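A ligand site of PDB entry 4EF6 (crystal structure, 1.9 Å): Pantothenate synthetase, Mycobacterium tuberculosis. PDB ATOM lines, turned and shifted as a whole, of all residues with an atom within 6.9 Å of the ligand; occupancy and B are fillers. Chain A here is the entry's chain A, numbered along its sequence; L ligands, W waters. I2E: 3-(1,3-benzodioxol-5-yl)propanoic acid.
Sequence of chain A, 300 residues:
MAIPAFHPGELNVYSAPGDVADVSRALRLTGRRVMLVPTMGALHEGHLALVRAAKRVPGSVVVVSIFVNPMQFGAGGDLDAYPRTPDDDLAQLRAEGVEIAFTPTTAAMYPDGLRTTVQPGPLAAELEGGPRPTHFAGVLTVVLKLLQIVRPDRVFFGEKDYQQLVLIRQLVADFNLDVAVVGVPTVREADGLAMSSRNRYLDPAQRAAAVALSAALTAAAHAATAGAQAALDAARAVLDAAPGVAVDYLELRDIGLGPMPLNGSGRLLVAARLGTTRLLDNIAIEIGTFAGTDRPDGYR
An oxygen (O2) of the ligand is in salt-bridge range of the side-chain amino group (NZ) of Lys 160 (2.4 Å). O1 of the ligand is in hydrogen-bond range of NE2 of His 44 (2.8 Å). OG of Ser 196 is in hydrogen-bond range of O2 of the ligand (2.8 Å). An oxygen (O1) of the ligand sits at hydrogen-bond distance from the backbone NH (N) of Ser 197, at 3.0 Å. OG of Ser 197 is in hydrogen-bond range of O1 of the ligand (3.4 Å). An oxygen (O4) of the ligand lies within hydrogen-bond range of the backbone NH of Val 187 (3.1 Å).
NZ of Lys 160 is in salt-bridge range of OD1 of Asp 161, at 3.1 Å. OG1 of Thr 186 is in hydrogen-bond range of N of Lys 160. A ring nitrogen (NE2) of His 44 lies within hydrogen-bond range of the backbone NH (N) of Ser 197, at 3.4 Å. N of Gly 46 lies within hydrogen-bond range of ND1 of His 44 (2.9 Å). The backbone NH (N) of His 44 sits at hydrogen-bond distance from a ring nitrogen (ND1) of His 47. The side-chain hydroxyl (OG) of Ser 196 sits close to the backbone NH (N) of Arg 198 (3.0 Å). The backbone carbonyl oxygen of Ala 42 is in hydrogen-bond range of the side-chain hydroxyl of Ser 197. The backbone carbonyl oxygen (O) of Val 187 sits at hydrogen-bond distance from the backbone NH (N) of Met 195, 2.8 Å away.
O of Gly 46 lies close to O3 of the ligand. Merely in contact with the ligand: Met 195 (3.2 Å), Asp 161 (3.2 Å), Gly 158 (3.3 Å), Leu 50 (3.3 Å), Pro 185 (3.5 Å), His 47 (3.5 Å) and Thr 186 (3.5 Å). Hydrophobic or aromatic side chains within 4 Å of the ligand: His 44, His 47, Leu 50 and Val 187. 13 residues have an atom within 4 Å of the ligand: His 44, Gly 46, His 47, Leu 50, Gly 158, Lys 160, Asp 161, Pro 185, Thr 186, Val 187, Met 195, Ser 196 and Ser 197.
Water W1 lies within hydrogen-bond range of the side-chain carboxylate of Asp 161 (3.1 Å) and the backbone carbonyl oxygen of Gly 158 (3.4 Å).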
ATOM      1  N   GLY A  41       7.902 -28.949 -22.820  1.00  0.00           N
ATOM      2  CA  GLY A  41       7.486 -28.410 -21.513  1.00  0.00           C
ATOM      3  C   GLY A  41       7.339 -26.852 -21.470  1.00  0.00           C
ATOM      4  O   GLY A  41       7.174 -26.189 -22.509  1.00  0.00           O
ATOM      5  N   ALA A  42       7.365 -26.288 -20.254  1.00  0.00           N
ATOM      6  CA  ALA A  42       7.107 -24.846 -20.050  1.00  0.00           C
ATOM      7  C   ALA A  42       5.765 -24.472 -20.690  1.00  0.00           C
ATOM      8  O   ALA A  42       5.657 -23.527 -21.479  1.00  0.00           O
ATOM      9  CB  ALA A  42       8.243 -23.997 -20.657  1.00  0.00           C
ATOM     10  N   HIS A  44       2.059 -23.425 -21.643  1.00  0.00           N
ATOM     11  CA  HIS A  44       1.238 -22.239 -21.487  1.00  0.00           C
ATOM     12  C   HIS A  44      -0.058 -22.487 -22.275  1.00  0.00           C
ATOM     13  O   HIS A  44      -0.302 -23.588 -22.737  1.00  0.00           O
ATOM     14  CB  HIS A  44       2.001 -21.027 -22.088  1.00  0.00           C
ATOM     15  CG  HIS A  44       2.586 -21.277 -23.457  1.00  0.00           C
ATOM     16  ND1 HIS A  44       1.809 -21.375 -24.600  1.00  0.00           N
ATOM     17  CD2 HIS A  44       3.880 -21.367 -23.876  1.00  0.00           C
ATOM     18  CE1 HIS A  44       2.599 -21.546 -25.663  1.00  0.00           C
ATOM     19  NE2 HIS A  44       3.856 -21.563 -25.243  1.00  0.00           N
ATOM     20  N   GLU A  45      -0.897 -21.465 -22.436  1.00  0.00           N
ATOM     21  CA  GLU A  45      -2.192 -21.644 -23.027  1.00  0.00           C
ATOM     22  C   GLU A  45      -2.119 -22.062 -24.504  1.00  0.00           C
ATOM     23  O   GLU A  45      -3.079 -22.654 -25.008  1.00  0.00           O
ATOM     24  CB  GLU A  45      -3.003 -20.353 -22.852  1.00  0.00           C
ATOM     25  CG  GLU A  45      -4.468 -20.513 -23.093  1.00  0.00           C
ATOM     26  CD  GLU A  45      -5.175 -21.240 -21.944  1.00  0.00           C
ATOM     27  OE1 GLU A  45      -4.688 -21.231 -20.783  1.00  0.00           O
ATOM     28  OE2 GLU A  45      -6.226 -21.847 -22.226  1.00  0.00           O
ATOM     29  N   GLY A  46      -1.040 -21.700 -25.217  1.00  0.00           N
ATOM     30  CA  GLY A  46      -0.855 -22.233 -26.563  1.00  0.00           C
ATOM     31  C   GLY A  46      -0.830 -23.780 -26.585  1.00  0.00           C
ATOM     32  O   GLY A  46      -1.511 -24.388 -27.378  1.00  0.00           O
ATOM     33  N   HIS A  47      -0.024 -24.400 -25.709  1.00  0.00           N
ATOM     34  CA  HIS A  47       0.000 -25.840 -25.572  1.00  0.00           C
ATOM     35  C   HIS A  47      -1.356 -26.348 -25.106  1.00  0.00           C
ATOM     36  O   HIS A  47      -1.757 -27.417 -25.530  1.00  0.00           O
ATOM     37  CB  HIS A  47       1.049 -26.279 -24.519  1.00  0.00           C
ATOM     38  CG  HIS A  47       2.454 -25.890 -24.859  1.00  0.00           C
ATOM     39  ND1 HIS A  47       3.139 -24.927 -24.158  1.00  0.00           N
ATOM     40  CD2 HIS A  47       3.323 -26.368 -25.779  1.00  0.00           C
ATOM     41  CE1 HIS A  47       4.364 -24.824 -24.647  1.00  0.00           C
ATOM     42  NE2 HIS A  47       4.490 -25.669 -25.641  1.00  0.00           N
ATOM     43  N   LEU A  48      -2.110 -25.588 -24.305  1.00  0.00           N
ATOM     44  CA  LEU A  48      -3.424 -26.179 -23.802  1.00  0.00           C
ATOM     45  C   LEU A  48      -4.439 -26.237 -24.963  1.00  0.00           C
ATOM     46  O   LEU A  48      -5.288 -27.134 -25.099  1.00  0.00           O
ATOM     47  CB  LEU A  48      -3.935 -25.402 -22.576  1.00  0.00           C
ATOM     48  CG  LEU A  48      -2.897 -25.323 -21.422  1.00  0.00           C
ATOM     49  CD1 LEU A  48      -3.454 -24.641 -20.136  1.00  0.00           C
ATOM     50  CD2 LEU A  48      -2.389 -26.673 -21.074  1.00  0.00           C
ATOM     51  N   ALA A  49      -4.256 -25.338 -25.942  1.00  0.00           N
ATOM     52  CA  ALA A  49      -5.139 -25.411 -27.072  1.00  0.00           C
ATOM     53  C   ALA A  49      -4.855 -26.707 -27.847  1.00  0.00           C
ATOM     54  O   ALA A  49      -5.778 -27.319 -28.379  1.00  0.00           O
ATOM     55  CB  ALA A  49      -5.010 -24.181 -27.988  1.00  0.00           C
ATOM     56  N   LEU A  50      -3.576 -27.097 -27.908  1.00  0.00           N
ATOM     57  CA  LEU A  50      -3.198 -28.335 -28.569  1.00  0.00           C
ATOM     58  C   LEU A  50      -3.845 -29.509 -27.804  1.00  0.00           C
ATOM     59  O   LEU A  50      -4.448 -30.383 -28.421  1.00  0.00           O
ATOM     60  CB  LEU A  50      -1.660 -28.515 -28.641  1.00  0.00           C
ATOM     61  CG  LEU A  50      -0.773 -27.393 -29.249  1.00  0.00           C
ATOM     62  CD1 LEU A  50       0.725 -27.786 -29.291  1.00  0.00           C
ATOM     63  CD2 LEU A  50      -1.277 -27.012 -30.652  1.00  0.00           C
ATOM     64  N   TYR A  82      16.893 -22.939 -21.703  1.00  0.00           N
ATOM     65  CA  TYR A  82      15.484 -23.276 -21.963  1.00  0.00           C
ATOM     66  C   TYR A  82      14.666 -23.389 -20.644  1.00  0.00           C
ATOM     67  O   TYR A  82      15.154 -24.000 -19.704  1.00  0.00           O
ATOM     68  CB  TYR A  82      15.337 -24.547 -22.824  1.00  0.00           C
ATOM     69  CG  TYR A  82      14.048 -24.517 -23.538  1.00  0.00           C
ATOM     70  CD1 TYR A  82      13.927 -23.800 -24.739  1.00  0.00           C
ATOM     71  CD2 TYR A  82      12.913 -25.161 -23.004  1.00  0.00           C
ATOM     72  CE1 TYR A  82      12.653 -23.716 -25.427  1.00  0.00           C
ATOM     73  CE2 TYR A  82      11.643 -25.074 -23.651  1.00  0.00           C
ATOM     74  CZ  TYR A  82      11.553 -24.355 -24.880  1.00  0.00           C
ATOM     75  OH  TYR A  82      10.369 -24.257 -25.539  1.00  0.00           O
ATOM     76  N   PHE A 157       0.501 -29.852 -33.647  1.00  0.00           N
ATOM     77  CA  PHE A 157       1.508 -28.785 -33.503  1.00  0.00           C
ATOM     78  C   PHE A 157       0.832 -27.384 -33.681  1.00  0.00           C
ATOM     79  O   PHE A 157      -0.152 -27.252 -34.420  1.00  0.00           O
ATOM     80  CB  PHE A 157       2.612 -28.940 -34.568  1.00  0.00           C
ATOM     81  CG  PHE A 157       3.508 -30.126 -34.344  1.00  0.00           C
ATOM     82  CD1 PHE A 157       4.665 -29.992 -33.568  1.00  0.00           C
ATOM     83  CD2 PHE A 157       3.241 -31.357 -34.940  1.00  0.00           C
ATOM     84  CE1 PHE A 157       5.505 -31.121 -33.314  1.00  0.00           C
ATOM     85  CE2 PHE A 157       4.087 -32.454 -34.744  1.00  0.00           C
ATOM     86  CZ  PHE A 157       5.216 -32.345 -33.902  1.00  0.00           C
ATOM     87  N   GLY A 158       1.391 -26.347 -33.044  1.00  0.00           N
ATOM     88  CA  GLY A 158       0.899 -24.995 -33.240  1.00  0.00           C
ATOM     89  C   GLY A 158       1.294 -24.470 -34.613  1.00  0.00           C
ATOM     90  O   GLY A 158       2.370 -24.787 -35.099  1.00  0.00           O
ATOM     91  N   GLU A 159       0.470 -23.611 -35.209  1.00  0.00           N
ATOM     92  CA  GLU A 159       0.892 -22.763 -36.373  1.00  0.00           C
ATOM     93  C   GLU A 159       1.961 -21.707 -36.044  1.00  0.00           C
ATOM     94  O   GLU A 159       2.601 -21.148 -36.920  1.00  0.00           O
ATOM     95  CB  GLU A 159      -0.333 -22.079 -36.958  1.00  0.00           C
ATOM     96  CG  GLU A 159      -1.123 -23.070 -37.782  1.00  0.00           C
ATOM     97  CD  GLU A 159      -2.423 -22.523 -38.394  1.00  0.00           C
ATOM     98  OE1 GLU A 159      -2.634 -21.293 -38.384  1.00  0.00           O
ATOM     99  OE2 GLU A 159      -3.214 -23.393 -38.805  1.00  0.00           O
ATOM    100  N   LYS A 160       2.131 -21.418 -34.757  1.00  0.00           N
ATOM    101  CA  LYS A 160       3.090 -20.422 -34.331  1.00  0.00           C
ATOM    102  C   LYS A 160       4.518 -20.689 -34.913  1.00  0.00           C
ATOM    103  O   LYS A 160       5.142 -19.820 -35.504  1.00  0.00           O
ATOM    104  CB  LYS A 160       3.114 -20.348 -32.782  1.00  0.00           C
ATOM    105  CG  LYS A 160       3.802 -19.044 -32.254  1.00  0.00           C
ATOM    106  CD  LYS A 160       5.296 -19.102 -32.220  1.00  0.00           C
ATOM    107  CE  LYS A 160       5.698 -19.834 -30.995  1.00  0.00           C
ATOM    108  NZ  LYS A 160       7.176 -20.042 -30.783  1.00  0.00           N
ATOM    109  N   ASP A 161       5.006 -21.908 -34.758  1.00  0.00           N
ATOM    110  CA  ASP A 161       6.274 -22.266 -35.361  1.00  0.00           C
ATOM    111  C   ASP A 161       5.923 -22.883 -36.711  1.00  0.00           C
ATOM    112  O   ASP A 161       5.937 -24.102 -36.919  1.00  0.00           O
ATOM    113  CB  ASP A 161       6.983 -23.232 -34.461  1.00  0.00           C
ATOM    114  CG  ASP A 161       7.382 -22.599 -33.157  1.00  0.00           C
ATOM    115  OD1 ASP A 161       8.158 -21.661 -33.215  1.00  0.00           O
ATOM    116  OD2 ASP A 161       6.831 -22.955 -32.116  1.00  0.00           O
ATOM    117  N   GLN A 164       8.474 -25.006 -38.835  1.00  0.00           N
ATOM    118  CA  GLN A 164       8.522 -26.303 -38.221  1.00  0.00           C
ATOM    119  C   GLN A 164       7.310 -27.192 -38.610  1.00  0.00           C
ATOM    120  O   GLN A 164       7.473 -28.369 -38.963  1.00  0.00           O
ATOM    121  CB  GLN A 164       8.667 -26.146 -36.705  1.00  0.00           C
ATOM    122  CG  GLN A 164       8.561 -27.503 -35.978  1.00  0.00           C
ATOM    123  CD  GLN A 164       8.545 -27.344 -34.487  1.00  0.00           C
ATOM    124  OE1 GLN A 164       9.590 -27.149 -33.866  1.00  0.00           O
ATOM    125  NE2 GLN A 164       7.322 -27.350 -33.889  1.00  0.00           N
ATOM    126  N   VAL A 184      -2.683 -26.393 -35.255  1.00  0.00           N
ATOM    127  CA  VAL A 184      -3.623 -25.641 -34.431  1.00  0.00           C
ATOM    128  C   VAL A 184      -3.290 -24.145 -34.482  1.00  0.00           C
ATOM    129  O   VAL A 184      -2.106 -23.783 -34.320  1.00  0.00           O
ATOM    130  CB  VAL A 184      -3.570 -26.150 -32.977  1.00  0.00           C
ATOM    131  CG1 VAL A 184      -4.473 -25.323 -31.971  1.00  0.00           C
ATOM    132  CG2 VAL A 184      -3.968 -27.569 -32.965  1.00  0.00           C
ATOM    133  N   PRO A 185      -4.322 -23.273 -34.713  1.00  0.00           N
ATOM    134  CA  PRO A 185      -4.112 -21.822 -34.748  1.00  0.00           C
ATOM    135  C   PRO A 185      -3.348 -21.289 -33.541  1.00  0.00           C
ATOM    136  O   PRO A 185      -3.570 -21.737 -32.418  1.00  0.00           O
ATOM    137  CB  PRO A 185      -5.547 -21.263 -34.768  1.00  0.00           C
ATOM    138  CG  PRO A 185      -6.286 -22.356 -35.666  1.00  0.00           C
ATOM    139  CD  PRO A 185      -5.706 -23.656 -35.116  1.00  0.00           C
ATOM    140  N   THR A 186      -2.429 -20.383 -33.801  1.00  0.00           N
ATOM    141  CA  THR A 186      -1.707 -19.644 -32.732  1.00  0.00           C
ATOM    142  C   THR A 186      -2.627 -19.009 -31.633  1.00  0.00           C
ATOM    143  O   THR A 186      -3.611 -18.337 -31.956  1.00  0.00           O
ATOM    144  CB  THR A 186      -0.815 -18.545 -33.411  1.00  0.00           C
ATOM    145  OG1 THR A 186       0.131 -19.183 -34.317  1.00  0.00           O
ATOM    146  CG2 THR A 186      -0.091 -17.655 -32.370  1.00  0.00           C
ATOM    147  N   VAL A 187      -2.325 -19.250 -30.357  1.00  0.00           N
ATOM    148  CA  VAL A 187      -3.098 -18.671 -29.270  1.00  0.00           C
ATOM    149  C   VAL A 187      -2.413 -17.342 -28.941  1.00  0.00           C
ATOM    150  O   VAL A 187      -1.213 -17.276 -28.892  1.00  0.00           O
ATOM    151  CB  VAL A 187      -3.199 -19.632 -28.017  1.00  0.00           C
ATOM    152  CG1 VAL A 187      -3.995 -18.951 -26.843  1.00  0.00           C
ATOM    153  CG2 VAL A 187      -3.787 -20.966 -28.407  1.00  0.00           C
ATOM    154  N   ARG A 188      -3.196 -16.270 -28.802  1.00  0.00           N
ATOM    155  CA  ARG A 188      -2.627 -14.926 -28.604  1.00  0.00           C
ATOM    156  C   ARG A 188      -3.041 -14.289 -27.269  1.00  0.00           C
ATOM    157  O   ARG A 188      -4.104 -14.584 -26.781  1.00  0.00           O
ATOM    158  CB  ARG A 188      -2.990 -13.982 -29.757  1.00  0.00           C
ATOM    159  CG  ARG A 188      -2.490 -14.512 -31.126  1.00  0.00           C
ATOM    160  CD  ARG A 188      -2.947 -13.655 -32.305  1.00  0.00           C
ATOM    161  NE  ARG A 188      -2.342 -14.211 -33.506  1.00  0.00           N
ATOM    162  CZ  ARG A 188      -1.095 -13.980 -33.922  1.00  0.00           C
ATOM    163  NH1 ARG A 188      -0.273 -13.149 -33.240  1.00  0.00           N
ATOM    164  NH2 ARG A 188      -0.633 -14.572 -35.048  1.00  0.00           N
ATOM    165  N   ALA A 194       1.699 -13.304 -29.868  1.00  0.00           N
ATOM    166  CA  ALA A 194       1.630 -14.788 -30.005  1.00  0.00           C
ATOM    167  C   ALA A 194       2.092 -15.438 -28.678  1.00  0.00           C
ATOM    168  O   ALA A 194       3.136 -15.028 -28.171  1.00  0.00           O
ATOM    169  CB  ALA A 194       2.498 -15.280 -31.167  1.00  0.00           C
ATOM    170  N   MET A 195       1.338 -16.384 -28.115  1.00  0.00           N
ATOM    171  CA  MET A 195       1.827 -17.185 -26.949  1.00  0.00           C
ATOM    172  C   MET A 195       3.166 -17.885 -27.241  1.00  0.00           C
ATOM    173  O   MET A 195       3.355 -18.456 -28.308  1.00  0.00           O
ATOM    174  CB  MET A 195       0.824 -18.264 -26.549  1.00  0.00           C
ATOM    175  CG  MET A 195      -0.503 -17.743 -25.998  1.00  0.00           C
ATOM    176  SD  MET A 195      -0.326 -17.218 -24.309  1.00  0.00           S
ATOM    177  CE  MET A 195      -2.033 -16.759 -23.846  1.00  0.00           C
ATOM    178  N   SER A 196       4.114 -17.820 -26.298  1.00  0.00           N
ATOM    179  CA  SER A 196       5.379 -18.547 -26.478  1.00  0.00           C
ATOM    180  C   SER A 196       6.057 -18.661 -25.129  1.00  0.00           C
ATOM    181  O   SER A 196       5.909 -17.769 -24.264  1.00  0.00           O
ATOM    182  CB  SER A 196       6.327 -17.789 -27.432  1.00  0.00           C
ATOM    183  OG  SER A 196       7.586 -18.440 -27.415  1.00  0.00           O
ATOM    184  N   SER A 197       6.783 -19.773 -24.944  1.00  0.00           N
ATOM    185  CA  SER A 197       7.543 -19.988 -23.707  1.00  0.00           C
ATOM    186  C   SER A 197       8.630 -18.929 -23.588  1.00  0.00           C
ATOM    187  O   SER A 197       9.120 -18.686 -22.498  1.00  0.00           O
ATOM    188  CB  SER A 197       8.204 -21.402 -23.694  1.00  0.00           C
ATOM    189  OG  SER A 197       7.229 -22.441 -23.691  1.00  0.00           O
ATOM    190  N   ARG A 198       8.995 -18.309 -24.714  1.00  0.00           N
ATOM    191  CA  ARG A 198       9.965 -17.221 -24.713  1.00  0.00           C
ATOM    192  C   ARG A 198       9.434 -15.838 -24.255  1.00  0.00           C
ATOM    193  O   ARG A 198      10.258 -14.937 -23.979  1.00  0.00           O
ATOM    194  CB  ARG A 198      10.654 -17.078 -26.082  1.00  0.00           C
ATOM    195  CG  ARG A 198      11.359 -18.383 -26.619  1.00  0.00           C
ATOM    196  CD  ARG A 198      11.668 -19.470 -25.512  1.00  0.00           C
ATOM    197  NE  ARG A 198      13.049 -19.915 -25.639  1.00  0.00           N
ATOM    198  CZ  ARG A 198      13.528 -20.532 -26.725  1.00  0.00           C
ATOM    199  NH1 ARG A 198      12.702 -20.825 -27.727  1.00  0.00           N
ATOM    200  NH2 ARG A 198      14.833 -20.858 -26.799  1.00  0.00           N
HETATM  201  C4  I2E L   1       0.923 -21.959 -29.679  1.00  0.00           C
HETATM  202  C5  I2E L   1       1.928 -21.152 -29.234  1.00  0.00           C
HETATM  203  C6  I2E L   1       3.153 -21.712 -28.841  1.00  0.00           C
HETATM  204  C3  I2E L   1       1.090 -23.323 -29.765  1.00  0.00           C
HETATM  205  C2  I2E L   1       2.275 -23.921 -29.418  1.00  0.00           C
HETATM  206  C1  I2E L   1       3.350 -23.130 -28.969  1.00  0.00           C
HETATM  207  C7  I2E L   1       4.550 -23.741 -28.561  1.00  0.00           C
HETATM  208  C8  I2E L   1       5.836 -22.974 -29.042  1.00  0.00           C
HETATM  209  C9  I2E L   1       6.352 -21.894 -28.034  1.00  0.00           C
HETATM  210  O1  I2E L   1       6.098 -21.966 -26.813  1.00  0.00           O
HETATM  211  C20 I2E L   1      -1.056 -22.857 -30.337  1.00  0.00           C
HETATM  212  O2  I2E L   1       6.993 -20.984 -28.539  1.00  0.00           O
HETATM  213  O4  I2E L   1      -0.336 -21.592 -30.122  1.00  0.00           O
HETATM  214  O3  I2E L   1      -0.057 -23.923 -30.245  1.00  0.00           O
HETATM  215  O   HOH W   1       3.849 -23.604 -32.267  1.00  0.00           O
